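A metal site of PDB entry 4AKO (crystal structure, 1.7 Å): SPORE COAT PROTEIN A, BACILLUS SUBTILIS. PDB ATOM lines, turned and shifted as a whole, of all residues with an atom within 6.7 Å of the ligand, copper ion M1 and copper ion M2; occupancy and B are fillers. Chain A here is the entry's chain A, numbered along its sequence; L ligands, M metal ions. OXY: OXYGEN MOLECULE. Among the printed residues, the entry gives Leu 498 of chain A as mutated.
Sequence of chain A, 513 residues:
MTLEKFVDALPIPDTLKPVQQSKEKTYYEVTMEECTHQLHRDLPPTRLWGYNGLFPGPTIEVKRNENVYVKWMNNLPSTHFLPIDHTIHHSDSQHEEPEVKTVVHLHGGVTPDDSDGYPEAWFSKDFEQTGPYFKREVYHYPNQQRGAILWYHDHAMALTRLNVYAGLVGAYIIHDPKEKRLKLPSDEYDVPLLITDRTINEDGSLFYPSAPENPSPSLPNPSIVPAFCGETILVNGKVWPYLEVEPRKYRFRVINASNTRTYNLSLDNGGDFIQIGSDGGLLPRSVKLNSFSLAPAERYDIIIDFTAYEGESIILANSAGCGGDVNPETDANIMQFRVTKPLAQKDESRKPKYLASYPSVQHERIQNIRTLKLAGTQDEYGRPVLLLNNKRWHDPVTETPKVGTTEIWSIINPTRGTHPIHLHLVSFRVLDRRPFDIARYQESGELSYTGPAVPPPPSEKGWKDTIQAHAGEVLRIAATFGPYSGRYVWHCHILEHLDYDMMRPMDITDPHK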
ATOM      1  N   HIS A 105      19.428  -8.217  25.190  1.00  0.00           N
ATOM      2  CA  HIS A 105      18.730  -9.463  24.931  1.00  0.00           C
ATOM      3  C   HIS A 105      19.666 -10.449  24.235  1.00  0.00           C
ATOM      4  O   HIS A 105      20.266 -10.124  23.211  1.00  0.00           O
ATOM      5  CB  HIS A 105      17.509  -9.209  24.068  1.00  0.00           C
ATOM      6  CG  HIS A 105      16.858 -10.467  23.591  1.00  0.00           C
ATOM      7  ND1 HIS A 105      16.451 -11.452  24.472  1.00  0.00           N
ATOM      8  CD2 HIS A 105      16.567 -10.923  22.359  1.00  0.00           C
ATOM      9  CE1 HIS A 105      15.925 -12.460  23.794  1.00  0.00           C
ATOM     10  NE2 HIS A 105      15.988 -12.155  22.507  1.00  0.00           N
ATOM     11  N   LEU A 106      19.801 -11.640  24.810  1.00  0.00           N
ATOM     12  CA  LEU A 106      20.505 -12.737  24.150  1.00  0.00           C
ATOM     13  C   LEU A 106      19.501 -13.479  23.270  1.00  0.00           C
ATOM     14  O   LEU A 106      18.693 -14.284  23.759  1.00  0.00           O
ATOM     15  CB  LEU A 106      21.167 -13.672  25.167  1.00  0.00           C
ATOM     16  CG  LEU A 106      21.846 -14.927  24.574  1.00  0.00           C
ATOM     17  CD1 LEU A 106      22.938 -14.512  23.590  1.00  0.00           C
ATOM     18  CD2 LEU A 106      22.417 -15.819  25.669  1.00  0.00           C
ATOM     19  N   HIS A 107      19.552 -13.148  21.978  1.00  0.00           N
ATOM     20  CA  HIS A 107      18.607 -13.665  21.007  1.00  0.00           C
ATOM     21  C   HIS A 107      18.812 -15.168  20.786  1.00  0.00           C
ATOM     22  O   HIS A 107      19.866 -15.605  20.337  1.00  0.00           O
ATOM     23  CB  HIS A 107      18.752 -12.897  19.692  1.00  0.00           C
ATOM     24  CG  HIS A 107      17.697 -13.211  18.684  1.00  0.00           C
ATOM     25  ND1 HIS A 107      16.833 -12.254  18.195  1.00  0.00           N
ATOM     26  CD2 HIS A 107      17.358 -14.370  18.081  1.00  0.00           C
ATOM     27  CE1 HIS A 107      15.999 -12.815  17.338  1.00  0.00           C
ATOM     28  NE2 HIS A 107      16.300 -14.098  17.239  1.00  0.00           N
ATOM     29  N   GLY A 108      17.766 -15.944  21.103  1.00  0.00           N
ATOM     30  CA  GLY A 108      17.823 -17.396  21.058  1.00  0.00           C
ATOM     31  C   GLY A 108      18.130 -18.045  22.412  1.00  0.00           C
ATOM     32  O   GLY A 108      18.139 -19.272  22.538  1.00  0.00           O
ATOM     33  N   ASP A 116      16.387 -12.055  30.384  1.00  0.00           N
ATOM     34  CA  ASP A 116      16.090 -12.155  28.951  1.00  0.00           C
ATOM     35  C   ASP A 116      16.187 -10.816  28.203  1.00  0.00           C
ATOM     36  O   ASP A 116      16.209 -10.788  26.976  1.00  0.00           O
ATOM     37  CB  ASP A 116      14.713 -12.795  28.736  1.00  0.00           C
ATOM     38  CG  ASP A 116      14.471 -13.181  27.287  1.00  0.00           C
ATOM     39  OD1 ASP A 116      15.365 -13.811  26.689  1.00  0.00           O
ATOM     40  OD2 ASP A 116      13.397 -12.830  26.767  1.00  0.00           O
ATOM     41  N   GLY A 117      16.259  -9.716  28.949  1.00  0.00           N
ATOM     42  CA  GLY A 117      16.330  -8.393  28.343  1.00  0.00           C
ATOM     43  C   GLY A 117      14.962  -7.852  27.963  1.00  0.00           C
ATOM     44  O   GLY A 117      14.763  -7.359  26.852  1.00  0.00           O
ATOM     45  N   PRO A 119      11.952  -5.468  27.380  1.00  0.00           N
ATOM     46  CA  PRO A 119      12.052  -4.074  26.908  1.00  0.00           C
ATOM     47  C   PRO A 119      11.924  -3.043  28.031  1.00  0.00           C
ATOM     48  O   PRO A 119      12.526  -1.981  27.939  1.00  0.00           O
ATOM     49  CB  PRO A 119      10.876  -3.947  25.927  1.00  0.00           C
ATOM     50  CG  PRO A 119      10.646  -5.349  25.446  1.00  0.00           C
ATOM     51  CD  PRO A 119      10.898  -6.205  26.648  1.00  0.00           C
ATOM     52  N   TRP A 151      22.887 -14.503  19.158  1.00  0.00           N
ATOM     53  CA  TRP A 151      23.501 -13.193  19.086  1.00  0.00           C
ATOM     54  C   TRP A 151      22.868 -12.300  20.118  1.00  0.00           C
ATOM     55  O   TRP A 151      21.778 -12.589  20.599  1.00  0.00           O
ATOM     56  CB  TRP A 151      23.422 -12.599  17.665  1.00  0.00           C
ATOM     57  CG  TRP A 151      22.073 -12.246  17.132  1.00  0.00           C
ATOM     58  CD1 TRP A 151      21.023 -13.102  16.882  1.00  0.00           C
ATOM     59  CD2 TRP A 151      21.649 -10.948  16.707  1.00  0.00           C
ATOM     60  NE1 TRP A 151      19.963 -12.397  16.352  1.00  0.00           N
ATOM     61  CE2 TRP A 151      20.327 -11.080  16.231  1.00  0.00           C
ATOM     62  CE3 TRP A 151      22.258  -9.686  16.686  1.00  0.00           C
ATOM     63  CZ2 TRP A 151      19.594  -9.982  15.734  1.00  0.00           C
ATOM     64  CZ3 TRP A 151      21.539  -8.597  16.195  1.00  0.00           C
ATOM     65  CH2 TRP A 151      20.215  -8.758  15.734  1.00  0.00           C
ATOM     66  N   HIS A 153      21.980  -8.220  21.502  1.00  0.00           N
ATOM     67  CA  HIS A 153      21.742  -6.862  21.015  1.00  0.00           C
ATOM     68  C   HIS A 153      20.853  -6.095  21.981  1.00  0.00           C
ATOM     69  O   HIS A 153      20.204  -6.696  22.848  1.00  0.00           O
ATOM     70  CB  HIS A 153      21.120  -6.873  19.603  1.00  0.00           C
ATOM     71  CG  HIS A 153      19.779  -7.548  19.524  1.00  0.00           C
ATOM     72  ND1 HIS A 153      18.610  -6.911  19.896  1.00  0.00           N
ATOM     73  CD2 HIS A 153      19.425  -8.779  19.084  1.00  0.00           C
ATOM     74  CE1 HIS A 153      17.593  -7.734  19.698  1.00  0.00           C
ATOM     75  NE2 HIS A 153      18.057  -8.872  19.208  1.00  0.00           N
ATOM     76  N   ASP A 154      20.831  -4.784  21.834  1.00  0.00           N
ATOM     77  CA  ASP A 154      19.974  -3.962  22.676  1.00  0.00           C
ATOM     78  C   ASP A 154      18.496  -4.219  22.427  1.00  0.00           C
ATOM     79  O   ASP A 154      18.102  -4.515  21.291  1.00  0.00           O
ATOM     80  CB  ASP A 154      20.263  -2.480  22.487  1.00  0.00           C
ATOM     81  CG  ASP A 154      19.598  -1.637  23.544  1.00  0.00           C
ATOM     82  OD1 ASP A 154      20.101  -1.624  24.679  1.00  0.00           O
ATOM     83  OD2 ASP A 154      18.537  -1.031  23.243  1.00  0.00           O
ATOM     84  N   HIS A 155      17.675  -4.083  23.460  1.00  0.00           N
ATOM     85  CA  HIS A 155      16.240  -4.324  23.351  1.00  0.00           C
ATOM     86  C   HIS A 155      15.412  -3.292  24.105  1.00  0.00           C
ATOM     87  O   HIS A 155      14.274  -3.552  24.483  1.00  0.00           O
ATOM     88  CB  HIS A 155      15.905  -5.742  23.865  1.00  0.00           C
ATOM     89  CG  HIS A 155      14.786  -6.423  23.129  1.00  0.00           C
ATOM     90  ND1 HIS A 155      13.526  -5.864  22.991  1.00  0.00           N
ATOM     91  CD2 HIS A 155      14.720  -7.630  22.515  1.00  0.00           C
ATOM     92  CE1 HIS A 155      12.756  -6.687  22.305  1.00  0.00           C
ATOM     93  NE2 HIS A 155      13.450  -7.773  22.015  1.00  0.00           N
ATOM     94  N   THR A 160      15.029   0.373  20.291  1.00  0.00           N
ATOM     95  CA  THR A 160      15.759  -0.768  19.749  1.00  0.00           C
ATOM     96  C   THR A 160      16.344  -0.481  18.361  1.00  0.00           C
ATOM     97  O   THR A 160      17.504  -0.807  18.099  1.00  0.00           O
ATOM     98  CB  THR A 160      14.879  -2.048  19.805  1.00  0.00           C
ATOM     99  OG1 THR A 160      14.531  -2.314  21.175  1.00  0.00           O
ATOM    100  CG2 THR A 160      15.613  -3.247  19.241  1.00  0.00           C
ATOM    101  N   ALA A 297      17.544 -11.012  12.026  1.00  0.00           N
ATOM    102  CA  ALA A 297      17.667 -11.929  13.183  1.00  0.00           C
ATOM    103  C   ALA A 297      17.750 -13.416  12.852  1.00  0.00           C
ATOM    104  O   ALA A 297      17.979 -14.229  13.755  1.00  0.00           O
ATOM    105  CB  ALA A 297      16.599 -11.668  14.238  1.00  0.00           C
ATOM    106  N   HIS A 422       9.563 -13.212  15.664  1.00  0.00           N
ATOM    107  CA  HIS A 422      10.425 -13.794  16.663  1.00  0.00           C
ATOM    108  C   HIS A 422       9.698 -14.036  17.978  1.00  0.00           C
ATOM    109  O   HIS A 422       9.017 -13.156  18.487  1.00  0.00           O
ATOM    110  CB  HIS A 422      11.631 -12.882  16.900  1.00  0.00           C
ATOM    111  CG  HIS A 422      12.542 -13.380  17.965  1.00  0.00           C
ATOM    112  ND1 HIS A 422      13.035 -14.665  17.960  1.00  0.00           N
ATOM    113  CD2 HIS A 422      13.054 -12.790  19.065  1.00  0.00           C
ATOM    114  CE1 HIS A 422      13.798 -14.845  19.017  1.00  0.00           C
ATOM    115  NE2 HIS A 422      13.821 -13.724  19.705  1.00  0.00           N
ATOM    116  N   LEU A 423       9.830 -15.260  18.514  1.00  0.00           N
ATOM    117  CA  LEU A 423       9.350 -15.577  19.861  1.00  0.00           C
ATOM    118  C   LEU A 423      10.558 -15.722  20.786  1.00  0.00           C
ATOM    119  O   LEU A 423      11.509 -16.432  20.455  1.00  0.00           O
ATOM    120  CB  LEU A 423       8.554 -16.889  19.874  1.00  0.00           C
ATOM    121  CG  LEU A 423       7.083 -16.847  19.468  1.00  0.00           C
ATOM    122  CD1 LEU A 423       6.911 -16.391  18.016  1.00  0.00           C
ATOM    123  CD2 LEU A 423       6.436 -18.212  19.664  1.00  0.00           C
ATOM    124  N   HIS A 424      10.517 -15.060  21.929  1.00  0.00           N
ATOM    125  CA  HIS A 424      11.561 -15.235  22.941  1.00  0.00           C
ATOM    126  C   HIS A 424      11.456 -16.603  23.601  1.00  0.00           C
ATOM    127  O   HIS A 424      10.442 -17.295  23.457  1.00  0.00           O
ATOM    128  CB  HIS A 424      11.482 -14.119  23.976  1.00  0.00           C
ATOM    129  CG  HIS A 424      12.054 -12.811  23.505  1.00  0.00           C
ATOM    130  ND1 HIS A 424      12.818 -11.999  24.310  1.00  0.00           N
ATOM    131  CD2 HIS A 424      11.980 -12.189  22.299  1.00  0.00           C
ATOM    132  CE1 HIS A 424      13.179 -10.926  23.632  1.00  0.00           C
ATOM    133  NE2 HIS A 424      12.683 -11.016  22.408  1.00  0.00           N
ATOM    134  N   THR A 466      13.130 -17.206  14.612  1.00  0.00           N
ATOM    135  CA  THR A 466      12.718 -16.048  13.841  1.00  0.00           C
ATOM    136  C   THR A 466      12.307 -16.557  12.469  1.00  0.00           C
ATOM    137  O   THR A 466      13.100 -17.215  11.799  1.00  0.00           O
ATOM    138  CB  THR A 466      13.859 -15.015  13.716  1.00  0.00           C
ATOM    139  OG1 THR A 466      14.350 -14.712  15.021  1.00  0.00           O
ATOM    140  CG2 THR A 466      13.362 -13.736  13.047  1.00  0.00           C
ATOM    141  N   VAL A 489       8.397 -11.948  25.515  1.00  0.00           N
ATOM    142  CA  VAL A 489       7.797 -11.152  24.446  1.00  0.00           C
ATOM    143  C   VAL A 489       7.783 -11.944  23.137  1.00  0.00           C
ATOM    144  O   VAL A 489       8.523 -12.926  22.980  1.00  0.00           O
ATOM    145  CB  VAL A 489       8.543  -9.776  24.229  1.00  0.00           C
ATOM    146  CG1 VAL A 489       8.551  -8.923  25.499  1.00  0.00           C
ATOM    147  CG2 VAL A 489       9.941  -9.969  23.706  1.00  0.00           C
ATOM    148  N   TRP A 490       6.947 -11.521  22.201  1.00  0.00           N
ATOM    149  CA  TRP A 490       7.041 -11.950  20.820  1.00  0.00           C
ATOM    150  C   TRP A 490       6.802 -10.723  19.944  1.00  0.00           C
ATOM    151  O   TRP A 490       6.088  -9.803  20.333  1.00  0.00           O
ATOM    152  CB  TRP A 490       6.073 -13.105  20.505  1.00  0.00           C
ATOM    153  CG  TRP A 490       4.620 -12.721  20.426  1.00  0.00           C
ATOM    154  CD1 TRP A 490       3.783 -12.426  21.460  1.00  0.00           C
ATOM    155  CD2 TRP A 490       3.833 -12.635  19.229  1.00  0.00           C
ATOM    156  NE1 TRP A 490       2.512 -12.144  20.982  1.00  0.00           N
ATOM    157  CE2 TRP A 490       2.525 -12.266  19.621  1.00  0.00           C
ATOM    158  CE3 TRP A 490       4.095 -12.830  17.863  1.00  0.00           C
ATOM    159  CZ2 TRP A 490       1.479 -12.090  18.700  1.00  0.00           C
ATOM    160  CZ3 TRP A 490       3.064 -12.656  16.940  1.00  0.00           C
ATOM    161  CH2 TRP A 490       1.775 -12.280  17.363  1.00  0.00           C
ATOM    162  N   HIS A 491       7.422 -10.696  18.769  1.00  0.00           N
ATOM    163  CA  HIS A 491       7.407  -9.478  17.953  1.00  0.00           C
ATOM    164  C   HIS A 491       7.958  -9.693  16.559  1.00  0.00           C
ATOM    165  O   HIS A 491       8.571 -10.709  16.251  1.00  0.00           O
ATOM    166  CB  HIS A 491       8.227  -8.376  18.644  1.00  0.00           C
ATOM    167  CG  HIS A 491       9.663  -8.737  18.883  1.00  0.00           C
ATOM    168  ND1 HIS A 491      10.661  -8.505  17.960  1.00  0.00           N
ATOM    169  CD2 HIS A 491      10.271  -9.306  19.955  1.00  0.00           C
ATOM    170  CE1 HIS A 491      11.814  -8.923  18.437  1.00  0.00           C
ATOM    171  NE2 HIS A 491      11.612  -9.404  19.652  1.00  0.00           N
ATOM    172  N   CYS A 492       7.722  -8.707  15.707  1.00  0.00           N
ATOM    173  CA  CYS A 492       8.407  -8.619  14.436  1.00  0.00           C
ATOM    174  C   CYS A 492       9.823  -8.115  14.682  1.00  0.00           C
ATOM    175  O   CYS A 492      10.019  -7.217  15.516  1.00  0.00           O
ATOM    176  CB  CYS A 492       7.660  -7.666  13.513  1.00  0.00           C
ATOM    177  SG  CYS A 492       8.506  -7.435  11.979  1.00  0.00           S
ATOM    178  N   HIS A 493      10.810  -8.687  13.984  1.00  0.00           N
ATOM    179  CA  HIS A 493      12.211  -8.276  14.155  1.00  0.00           C
ATOM    180  C   HIS A 493      12.689  -7.240  13.120  1.00  0.00           C
ATOM    181  O   HIS A 493      13.888  -6.956  13.004  1.00  0.00           O
ATOM    182  CB  HIS A 493      13.165  -9.498  14.246  1.00  0.00           C
ATOM    183  CG  HIS A 493      14.304  -9.333  15.220  1.00  0.00           C
ATOM    184  ND1 HIS A 493      15.371  -8.489  14.996  1.00  0.00           N
ATOM    185  CD2 HIS A 493      14.562  -9.950  16.409  1.00  0.00           C
ATOM    186  CE1 HIS A 493      16.218  -8.568  16.004  1.00  0.00           C
ATOM    187  NE2 HIS A 493      15.757  -9.451  16.878  1.00  0.00           N
ATOM    188  N   LEU A 495      13.111  -3.772  13.090  1.00  0.00           N
ATOM    189  CA  LEU A 495      13.192  -2.967  14.305  1.00  0.00           C
ATOM    190  C   LEU A 495      12.326  -1.712  14.251  1.00  0.00           C
ATOM    191  O   LEU A 495      11.793  -1.275  15.270  1.00  0.00           O
ATOM    192  CB  LEU A 495      14.650  -2.630  14.645  1.00  0.00           C
ATOM    193  CG  LEU A 495      15.548  -3.857  14.850  1.00  0.00           C
ATOM    194  CD1 LEU A 495      16.941  -3.406  15.286  1.00  0.00           C
ATOM    195  CD2 LEU A 495      14.966  -4.849  15.874  1.00  0.00           C
ATOM    196  N   LEU A 498       8.971  -3.156  15.255  1.00  0.00           N
ATOM    197  CA  LEU A 498       9.039  -3.486  16.672  1.00  0.00           C
ATOM    198  C   LEU A 498       8.757  -2.265  17.557  1.00  0.00           C
ATOM    199  O   LEU A 498       7.920  -2.329  18.453  1.00  0.00           O
ATOM    200  CB  LEU A 498      10.420  -4.095  16.997  1.00  0.00           C
ATOM    201  CG  LEU A 498      10.719  -4.748  18.347  1.00  0.00           C
ATOM    202  CD1 LEU A 498      12.051  -5.467  18.225  1.00  0.00           C
ATOM    203  CD2 LEU A 498      10.770  -3.749  19.489  1.00  0.00           C
ATOM    204  N   MET A 503       5.013  -5.441  18.863  1.00  0.00           N
ATOM    205  CA  MET A 503       5.559  -6.286  19.894  1.00  0.00           C
ATOM    206  C   MET A 503       4.526  -6.475  20.994  1.00  0.00           C
ATOM    207  O   MET A 503       3.836  -5.529  21.377  1.00  0.00           O
ATOM    208  CB  MET A 503       6.823  -5.645  20.475  1.00  0.00           C
ATOM    209  CG  MET A 503       7.422  -6.427  21.620  1.00  0.00           C
ATOM    210  SD  MET A 503       9.044  -5.865  22.148  1.00  0.00           S
ATOM    211  CE  MET A 503       8.661  -4.226  22.770  1.00  0.00           C
HETATM  212  O1  OXY L   1      14.904 -10.101  19.928  1.00  0.00           O
HETATM  213  O2  OXY L   1      14.751  -9.101  19.598  1.00  0.00           O
HETATM  214 CU    CU M   1      16.852 -10.267  18.399  1.00  0.00          CU
HETATM  215 CU    CU M   2      12.948  -9.502  21.125  1.00  0.00          CU
HETATM  216 CU    CU M   3      14.878 -12.762  21.019  1.00  0.00          CU
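Copper ion M2 is bound by NE2 of His 491 (2.0 Å).
A ring nitrogen (NE2) of His 424 is bound to copper ion M2, at 2.0 Å.
A ring nitrogen (NE2) of His 155 is bound to copper ion M2 (2.0 Å).
Copper ion M2 is bound by O1 of the ligand (2.4 Å).
The backbone carbonyl oxygen of His 491 is in hydrogen-bond range of the backbone NH of His 422 (2.8 Å).
A ring nitrogen (NE2) of His 107 sits close to a ring nitrogen (ND1) of His 422, at 3.4 Å.
The backbone carbonyl oxygen (O) of Trp 151 lies within hydrogen-bond range of the backbone NH (N) of His 107 (2.7 Å).
The side-chain hydroxyl (OG1) of Thr 466 lies within hydrogen-bond range of a ring nitrogen (NE2) of His 107 (3.0 Å).
The backbone carbonyl oxygen of Val 489 lies within hydrogen-bond range of the backbone NH of His 424 (3.1 Å).
OD2 of Asp 116 is in hydrogen-bond range of ND1 of His 424 (2.7 Å).
The backbone carbonyl oxygen (O) of His 153 sits at hydrogen-bond distance from the backbone NH (N) of His 105 (2.9 Å).
A ring nitrogen (ND1) of His 422 is in hydrogen-bond range of the side-chain hydroxyl (OG1) of Thr 466, 3.2 Å away.
His 422 touches copper ion M2.
Val 489 touches copper ion M2 (CG2 to CU, 3.99 Å).
Of the 25 residues printed, 5 come within 4 Å of copper ion M2.
The nearest printed residue that does not touch copper ion M2 is His 105 (4.1 Å).
Copper ion M1 is bound by a ring nitrogen (ND1) of His 107 (2.0 Å), a ring nitrogen (NE2) of His 153 (2.0 Å), a ring nitrogen (NE2) of His 493 (2.0 Å) and an oxygen (O1) of the ligand (2.5 Å).
Trp 151 touches copper ion M1 (CZ2 to CU, 3.8 Å).
Within 4 Å of copper ion M1: His 107, Trp 151, His 153 and His 493.
Along chain A the residues within 4 Å of copper ion M1 span positions 107 to 493.
The nearest printed residue that does not touch copper ion M1 is His 105 (4.02 Å).
NE2 of His 105 lies close to O1 of the ligand, at 3.5 Å.
Residues that only touch the ligand: His 422.
Hydrophobic or aromatic side chains that line the ligand: His 105, His 107, His 153, His 155, His 422, His 491 and His 493.
Of the 25 residues printed, 8 come within 4 Å of the ligand.
The nearest printed residue that does not touch the ligand is Leu 498 (4.7 Å).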
